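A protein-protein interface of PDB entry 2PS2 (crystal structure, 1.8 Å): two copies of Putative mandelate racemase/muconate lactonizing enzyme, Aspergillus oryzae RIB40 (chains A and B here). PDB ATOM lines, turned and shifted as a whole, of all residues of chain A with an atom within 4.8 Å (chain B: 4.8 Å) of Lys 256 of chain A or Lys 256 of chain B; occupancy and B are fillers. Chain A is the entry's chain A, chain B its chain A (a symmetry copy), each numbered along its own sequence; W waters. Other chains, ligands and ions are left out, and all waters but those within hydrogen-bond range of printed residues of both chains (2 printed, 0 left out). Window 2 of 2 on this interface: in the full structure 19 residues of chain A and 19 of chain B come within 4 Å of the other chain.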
ATOM      1  N   TRP A 228      13.810  13.114  15.596  1.00  0.00           N
ATOM      2  CA  TRP A 228      13.031  13.544  16.739  1.00  0.00           C
ATOM      3  C   TRP A 228      12.806  15.064  16.693  1.00  0.00           C
ATOM      4  O   TRP A 228      11.676  15.531  16.844  1.00  0.00           O
ATOM      5  CB  TRP A 228      13.766  13.140  18.020  1.00  0.00           C
ATOM      6  CG  TRP A 228      12.880  12.981  19.211  1.00  0.00           C
ATOM      7  CD1 TRP A 228      12.360  13.979  19.985  1.00  0.00           C
ATOM      8  CD2 TRP A 228      12.379  11.753  19.749  1.00  0.00           C
ATOM      9  NE1 TRP A 228      11.565  13.449  20.971  1.00  0.00           N
ATOM     10  CE2 TRP A 228      11.557  12.085  20.850  1.00  0.00           C
ATOM     11  CE3 TRP A 228      12.541  10.403  19.411  1.00  0.00           C
ATOM     12  CZ2 TRP A 228      10.898  11.115  21.616  1.00  0.00           C
ATOM     13  CZ3 TRP A 228      11.885   9.435  20.176  1.00  0.00           C
ATOM     14  CH2 TRP A 228      11.074   9.801  21.265  1.00  0.00           C
ATOM     15  N   ARG A 229      13.869  15.832  16.453  1.00  0.00           N
ATOM     16  CA  ARG A 229      13.743  17.291  16.412  1.00  0.00           C
ATOM     17  C   ARG A 229      12.698  17.750  15.397  1.00  0.00           C
ATOM     18  O   ARG A 229      11.881  18.620  15.685  1.00  0.00           O
ATOM     19  CB  ARG A 229      15.083  17.952  16.071  1.00  0.00           C
ATOM     20  CG  ARG A 229      15.064  19.472  16.252  1.00  0.00           C
ATOM     21  CD  ARG A 229      16.177  20.133  15.438  1.00  0.00           C
ATOM     22  NE  ARG A 229      15.940  20.008  14.001  1.00  0.00           N
ATOM     23  CZ  ARG A 229      15.129  20.795  13.295  1.00  0.00           C
ATOM     24  NH1 ARG A 229      14.470  21.792  13.882  1.00  0.00           N
ATOM     25  NH2 ARG A 229      14.959  20.570  11.995  1.00  0.00           N
ATOM     26  N   MET A 252      12.936   3.197  26.562  1.00  0.00           N
ATOM     27  CA  MET A 252      13.481   4.502  26.926  1.00  0.00           C
ATOM     28  C   MET A 252      12.958   5.568  25.948  1.00  0.00           C
ATOM     29  O   MET A 252      12.711   6.717  26.332  1.00  0.00           O
ATOM     30  CB  MET A 252      15.014   4.482  26.902  1.00  0.00           C
ATOM     31  CG  MET A 252      15.687   3.537  27.907  1.00  0.00           C
ATOM     32  SD  MET A 252      15.768   1.795  27.385  1.00  0.00           S
ATOM     33  CE  MET A 252      15.416   0.992  28.907  1.00  0.00           C
ATOM     34  N   SER A 253      12.779   5.190  24.685  1.00  0.00           N
ATOM     35  CA  SER A 253      12.279   6.146  23.699  1.00  0.00           C
ATOM     36  C   SER A 253      10.807   6.463  23.958  1.00  0.00           C
ATOM     37  O   SER A 253      10.361   7.587  23.741  1.00  0.00           O
ATOM     38  CB  SER A 253      12.449   5.612  22.263  1.00  0.00           C
ATOM     39  OG  SER A 253      11.511   4.577  21.968  1.00  0.00           O
ATOM     40  N   ILE A 254      10.052   5.476  24.432  1.00  0.00           N
ATOM     41  CA  ILE A 254       8.633   5.699  24.687  1.00  0.00           C
ATOM     42  C   ILE A 254       8.467   6.703  25.823  1.00  0.00           C
ATOM     43  O   ILE A 254       7.610   7.590  25.764  1.00  0.00           O
ATOM     44  CB  ILE A 254       7.911   4.385  25.041  1.00  0.00           C
ATOM     45  CG1 ILE A 254       8.232   3.312  23.987  1.00  0.00           C
ATOM     46  CG2 ILE A 254       6.417   4.638  25.148  1.00  0.00           C
ATOM     47  CD1 ILE A 254       8.027   3.753  22.526  1.00  0.00           C
ATOM     48  N   VAL A 255       9.289   6.568  26.859  1.00  0.00           N
ATOM     49  CA  VAL A 255       9.232   7.501  27.975  1.00  0.00           C
ATOM     50  C   VAL A 255       9.597   8.900  27.474  1.00  0.00           C
ATOM     51  O   VAL A 255       9.071   9.901  27.966  1.00  0.00           O
ATOM     52  CB  VAL A 255      10.201   7.075  29.107  1.00  0.00           C
ATOM     53  CG1 VAL A 255      10.361   8.202  30.112  1.00  0.00           C
ATOM     54  CG2 VAL A 255       9.653   5.834  29.805  1.00  0.00           C
ATOM     55  N   LYS A 256      10.481   8.975  26.484  1.00  0.00           N
ATOM     56  CA  LYS A 256      10.876  10.273  25.945  1.00  0.00           C
ATOM     57  C   LYS A 256       9.702  10.911  25.194  1.00  0.00           C
ATOM     58  O   LYS A 256       9.536  12.130  25.204  1.00  0.00           O
ATOM     59  CB  LYS A 256      12.089  10.117  25.020  1.00  0.00           C
ATOM     60  CG  LYS A 256      12.660  11.424  24.464  1.00  0.00           C
ATOM     61  CD  LYS A 256      13.026  12.400  25.564  1.00  0.00           C
ATOM     62  CE  LYS A 256      14.123  13.370  25.116  1.00  0.00           C
ATOM     63  NZ  LYS A 256      13.781  14.146  23.894  1.00  0.00           N
ATOM     64  N   ILE A 257       8.884  10.083  24.548  1.00  0.00           N
ATOM     65  CA  ILE A 257       7.724  10.597  23.829  1.00  0.00           C
ATOM     66  C   ILE A 257       6.816  11.303  24.835  1.00  0.00           C
ATOM     67  O   ILE A 257       6.327  12.402  24.587  1.00  0.00           O
ATOM     68  CB  ILE A 257       6.923   9.459  23.153  1.00  0.00           C
ATOM     69  CG1 ILE A 257       7.729   8.853  22.005  1.00  0.00           C
ATOM     70  CG2 ILE A 257       5.586   9.997  22.658  1.00  0.00           C
ATOM     71  CD1 ILE A 257       7.039   7.657  21.331  1.00  0.00           C
ATOM     72  N   LEU A 258       6.602  10.662  25.978  1.00  0.00           N
ATOM     73  CA  LEU A 258       5.763  11.219  27.030  1.00  0.00           C
ATOM     74  C   LEU A 258       6.382  12.472  27.645  1.00  0.00           C
ATOM     75  O   LEU A 258       5.685  13.444  27.929  1.00  0.00           O
ATOM     76  CB  LEU A 258       5.527  10.165  28.117  1.00  0.00           C
ATOM     77  CG  LEU A 258       4.459   9.122  27.781  1.00  0.00           C
ATOM     78  CD1 LEU A 258       4.559   7.923  28.720  1.00  0.00           C
ATOM     79  CD2 LEU A 258       3.091   9.782  27.893  1.00  0.00           C
ATOM     80  N   ALA A 259       7.693  12.453  27.845  1.00  0.00           N
ATOM     81  CA  ALA A 259       8.362  13.607  28.422  1.00  0.00           C
ATOM     82  C   ALA A 259       8.231  14.805  27.484  1.00  0.00           C
ATOM     83  O   ALA A 259       8.144  15.948  27.935  1.00  0.00           O
ATOM     84  CB  ALA A 259       9.826  13.292  28.667  1.00  0.00           C
ATOM     85  N   ASP A 260       8.212  14.545  26.180  1.00  0.00           N
ATOM     86  CA  ASP A 260       8.107  15.621  25.204  1.00  0.00           C
ATOM     87  C   ASP A 260       6.682  15.891  24.707  1.00  0.00           C
ATOM     88  O   ASP A 260       6.481  16.797  23.889  1.00  0.00           O
ATOM     89  CB  ASP A 260       8.998  15.327  23.984  1.00  0.00           C
ATOM     90  CG  ASP A 260      10.478  15.277  24.329  1.00  0.00           C
ATOM     91  OD1 ASP A 260      10.853  15.732  25.431  1.00  0.00           O
ATOM     92  OD2 ASP A 260      11.263  14.790  23.488  1.00  0.00           O
ATOM     93  N   TRP B 228      19.104  10.700  26.780  1.00  0.00           N
ATOM     94  CA  TRP B 228      18.924  12.107  26.487  1.00  0.00           C
ATOM     95  C   TRP B 228      18.014  12.760  27.540  1.00  0.00           C
ATOM     96  O   TRP B 228      18.352  13.809  28.090  1.00  0.00           O
ATOM     97  CB  TRP B 228      18.325  12.249  25.085  1.00  0.00           C
ATOM     98  CG  TRP B 228      18.611  13.559  24.426  1.00  0.00           C
ATOM     99  CD1 TRP B 228      17.987  14.750  24.666  1.00  0.00           C
ATOM    100  CD2 TRP B 228      19.616  13.822  23.441  1.00  0.00           C
ATOM    101  NE1 TRP B 228      18.543  15.739  23.893  1.00  0.00           N
ATOM    102  CE2 TRP B 228      19.545  15.199  23.132  1.00  0.00           C
ATOM    103  CE3 TRP B 228      20.571  13.031  22.788  1.00  0.00           C
ATOM    104  CZ2 TRP B 228      20.395  15.804  22.197  1.00  0.00           C
ATOM    105  CZ3 TRP B 228      21.417  13.635  21.854  1.00  0.00           C
ATOM    106  CH2 TRP B 228      21.320  15.009  21.571  1.00  0.00           C
ATOM    107  N   ARG B 229      16.879  12.130  27.843  1.00  0.00           N
ATOM    108  CA  ARG B 229      15.948  12.696  28.821  1.00  0.00           C
ATOM    109  C   ARG B 229      16.618  12.955  30.170  1.00  0.00           C
ATOM    110  O   ARG B 229      16.431  14.009  30.773  1.00  0.00           O
ATOM    111  CB  ARG B 229      14.746  11.771  29.040  1.00  0.00           C
ATOM    112  CG  ARG B 229      13.632  12.420  29.865  1.00  0.00           C
ATOM    113  CD  ARG B 229      12.727  11.360  30.493  1.00  0.00           C
ATOM    114  NE  ARG B 229      13.433  10.588  31.515  1.00  0.00           N
ATOM    115  CZ  ARG B 229      13.623  10.990  32.772  1.00  0.00           C
ATOM    116  NH1 ARG B 229      13.150  12.162  33.188  1.00  0.00           N
ATOM    117  NH2 ARG B 229      14.311  10.222  33.612  1.00  0.00           N
ATOM    118  N   MET B 252      23.056  14.723  13.083  1.00  0.00           N
ATOM    119  CA  MET B 252      21.676  15.017  13.460  1.00  0.00           C
ATOM    120  C   MET B 252      21.577  15.143  14.990  1.00  0.00           C
ATOM    121  O   MET B 252      20.802  15.952  15.512  1.00  0.00           O
ATOM    122  CB  MET B 252      20.727  13.918  12.966  1.00  0.00           C
ATOM    123  CG  MET B 252      20.637  13.746  11.444  1.00  0.00           C
ATOM    124  SD  MET B 252      21.979  12.763  10.704  1.00  0.00           S
ATOM    125  CE  MET B 252      22.272  13.681   9.235  1.00  0.00           C
ATOM    126  N   SER B 253      22.366  14.351  15.712  1.00  0.00           N
ATOM    127  CA  SER B 253      22.332  14.419  17.171  1.00  0.00           C
ATOM    128  C   SER B 253      22.958  15.722  17.663  1.00  0.00           C
ATOM    129  O   SER B 253      22.521  16.289  18.663  1.00  0.00           O
ATOM    130  CB  SER B 253      23.067  13.220  17.806  1.00  0.00           C
ATOM    131  OG  SER B 253      24.483  13.339  17.676  1.00  0.00           O
ATOM    132  N   ILE B 254      23.975  16.208  16.957  1.00  0.00           N
ATOM    133  CA  ILE B 254      24.634  17.440  17.375  1.00  0.00           C
ATOM    134  C   ILE B 254      23.664  18.610  17.247  1.00  0.00           C
ATOM    135  O   ILE B 254      23.603  19.482  18.119  1.00  0.00           O
ATOM    136  CB  ILE B 254      25.898  17.714  16.540  1.00  0.00           C
ATOM    137  CG1 ILE B 254      26.792  16.462  16.517  1.00  0.00           C
ATOM    138  CG2 ILE B 254      26.632  18.917  17.107  1.00  0.00           C
ATOM    139  CD1 ILE B 254      27.087  15.848  17.898  1.00  0.00           C
ATOM    140  N   VAL B 255      22.902  18.632  16.158  1.00  0.00           N
ATOM    141  CA  VAL B 255      21.920  19.688  15.963  1.00  0.00           C
ATOM    142  C   VAL B 255      20.869  19.603  17.073  1.00  0.00           C
ATOM    143  O   VAL B 255      20.340  20.624  17.517  1.00  0.00           O
ATOM    144  CB  VAL B 255      21.237  19.566  14.577  1.00  0.00           C
ATOM    145  CG1 VAL B 255      20.018  20.468  14.512  1.00  0.00           C
ATOM    146  CG2 VAL B 255      22.229  19.957  13.486  1.00  0.00           C
ATOM    147  N   LYS B 256      20.578  18.391  17.536  1.00  0.00           N
ATOM    148  CA  LYS B 256      19.592  18.226  18.599  1.00  0.00           C
ATOM    149  C   LYS B 256      20.132  18.802  19.913  1.00  0.00           C
ATOM    150  O   LYS B 256      19.378  19.346  20.719  1.00  0.00           O
ATOM    151  CB  LYS B 256      19.234  16.744  18.766  1.00  0.00           C
ATOM    152  CG  LYS B 256      18.136  16.448  19.790  1.00  0.00           C
ATOM    153  CD  LYS B 256      16.861  17.212  19.495  1.00  0.00           C
ATOM    154  CE  LYS B 256      15.630  16.498  20.062  1.00  0.00           C
ATOM    155  NZ  LYS B 256      15.700  16.244  21.526  1.00  0.00           N
ATOM    156  N   ILE B 257      21.442  18.689  20.123  1.00  0.00           N
ATOM    157  CA  ILE B 257      22.049  19.233  21.331  1.00  0.00           C
ATOM    158  C   ILE B 257      21.801  20.741  21.352  1.00  0.00           C
ATOM    159  O   ILE B 257      21.420  21.309  22.372  1.00  0.00           O
ATOM    160  CB  ILE B 257      23.575  18.983  21.365  1.00  0.00           C
ATOM    161  CG1 ILE B 257      23.864  17.492  21.542  1.00  0.00           C
ATOM    162  CG2 ILE B 257      24.205  19.798  22.487  1.00  0.00           C
ATOM    163  CD1 ILE B 257      25.359  17.144  21.501  1.00  0.00           C
ATOM    164  N   LEU B 258      22.015  21.382  20.208  1.00  0.00           N
ATOM    165  CA  LEU B 258      21.813  22.818  20.079  1.00  0.00           C
ATOM    166  C   LEU B 258      20.341  23.199  20.221  1.00  0.00           C
ATOM    167  O   LEU B 258      20.007  24.201  20.851  1.00  0.00           O
ATOM    168  CB  LEU B 258      22.349  23.297  18.726  1.00  0.00           C
ATOM    169  CG  LEU B 258      23.868  23.479  18.663  1.00  0.00           C
ATOM    170  CD1 LEU B 258      24.341  23.579  17.216  1.00  0.00           C
ATOM    171  CD2 LEU B 258      24.234  24.737  19.439  1.00  0.00           C
ATOM    172  N   ALA B 259      19.460  22.396  19.641  1.00  0.00           N
ATOM    173  CA  ALA B 259      18.037  22.683  19.731  1.00  0.00           C
ATOM    174  C   ALA B 259      17.584  22.605  21.187  1.00  0.00           C
ATOM    175  O   ALA B 259      16.690  23.341  21.606  1.00  0.00           O
ATOM    176  CB  ALA B 259      17.252  21.699  18.885  1.00  0.00           C
ATOM    177  N   ASP B 260      18.203  21.717  21.959  1.00  0.00           N
ATOM    178  CA  ASP B 260      17.831  21.554  23.358  1.00  0.00           C
ATOM    179  C   ASP B 260      18.706  22.338  24.343  1.00  0.00           C
ATOM    180  O   ASP B 260      18.462  22.282  25.555  1.00  0.00           O
ATOM    181  CB  ASP B 260      17.870  20.067  23.753  1.00  0.00           C
ATOM    182  CG  ASP B 260      16.856  19.225  22.996  1.00  0.00           C
ATOM    183  OD1 ASP B 260      15.940  19.804  22.373  1.00  0.00           O
ATOM    184  OD2 ASP B 260      16.974  17.981  23.036  1.00  0.00           O
HETATM  185  O   HOH W   1      12.782  16.619  22.228  1.00  0.00           O
HETATM  186  O   HOH W   2      15.138  16.761  24.577  1.00  0.00           O
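The side-chain amino group (NZ) of Lys 256 of chain B lies within salt-bridge range of the side-chain carboxylate (OD2) of Asp 260 of chain B (2.6 Å).
The side-chain carboxylate (OD2) of Asp 260 of chain A lies within salt-bridge range of the side-chain amino group (NZ) of Lys 256 of chain A, at 2.6 Å.
Printed residues of chain B that touch a printed residue of chain A: Arg 229, Val 255, Lys 256 and Ala 259.
Of the 11 printed residues of chain A, 4 touch a printed residue of chain B.
Along chain A the printed residues that touch a printed residue of chain B span positions 229 to 259.
Lys 256 of chain A touches two residues of chain B.
Lys 256 of chain B touches just these residues of chain A: Arg 229 and Lys 256.
Of the printed residues of chain A, Arg 229 of chain B touches Val 255, Lys 256 and Ala 259.
Of the printed residues of chain B, Arg 229 of chain A touches Val 255 (3.97 Å), Lys 256 (3.9 Å) and Ala 259 (3.9 Å).
Met 252 of chain B touches none of the printed residues of chain A.
Water W1 lies within hydrogen-bond range of the side-chain carboxylate (OD2) of Asp 260 of chain A (2.7 Å), the side-chain amino group (NZ) of Lys 256 of chain B (3.0 Å) and the side-chain amino group (NZ) of Lys 256 of chain A (3.1 Å).
Water W2 lies within hydrogen-bond range of OD2 of Asp 260 of chain B (2.7 Å), NZ of Lys 256 of chain A (3.0 Å) and NZ of Lys 256 of chain B (3.1 Å).
Among the printed residues, merely in contact across the chains: Lys 256 of chain A with Lys 256 of chain B, Arg 229 of chain A with Lys 256 of chain B, Lys 256 of chain A with Arg 229 of chain B, Ala 259 of chain A with Arg 229 of chain B, Arg 229 of chain A with Ala 259 of chain B, Val 255 of chain A with Arg 229 of chain B and Arg 229 of chain A with Val 255 of chain B.
Arg 229 of chain A touches Val 255 of chain B, and with the chains exchanged Val 255 of chain A touches Arg 229 of chain B.
Arg 229 of chain A touches Lys 256 of chain B, and with the chains exchanged Lys 256 of chain A touches Arg 229 of chain B.
Arg 229 of chain A touches Ala 259 of chain B, and with the chains exchanged Ala 259 of chain A touches Arg 229 of chain B.
Lys 256 of chain A touches its own counterpart, Lys 256 of chain B.
Positions printed for both chains: 228, 229, 252, 253, 254, 255, 256, 257, 258, 259 and 260.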
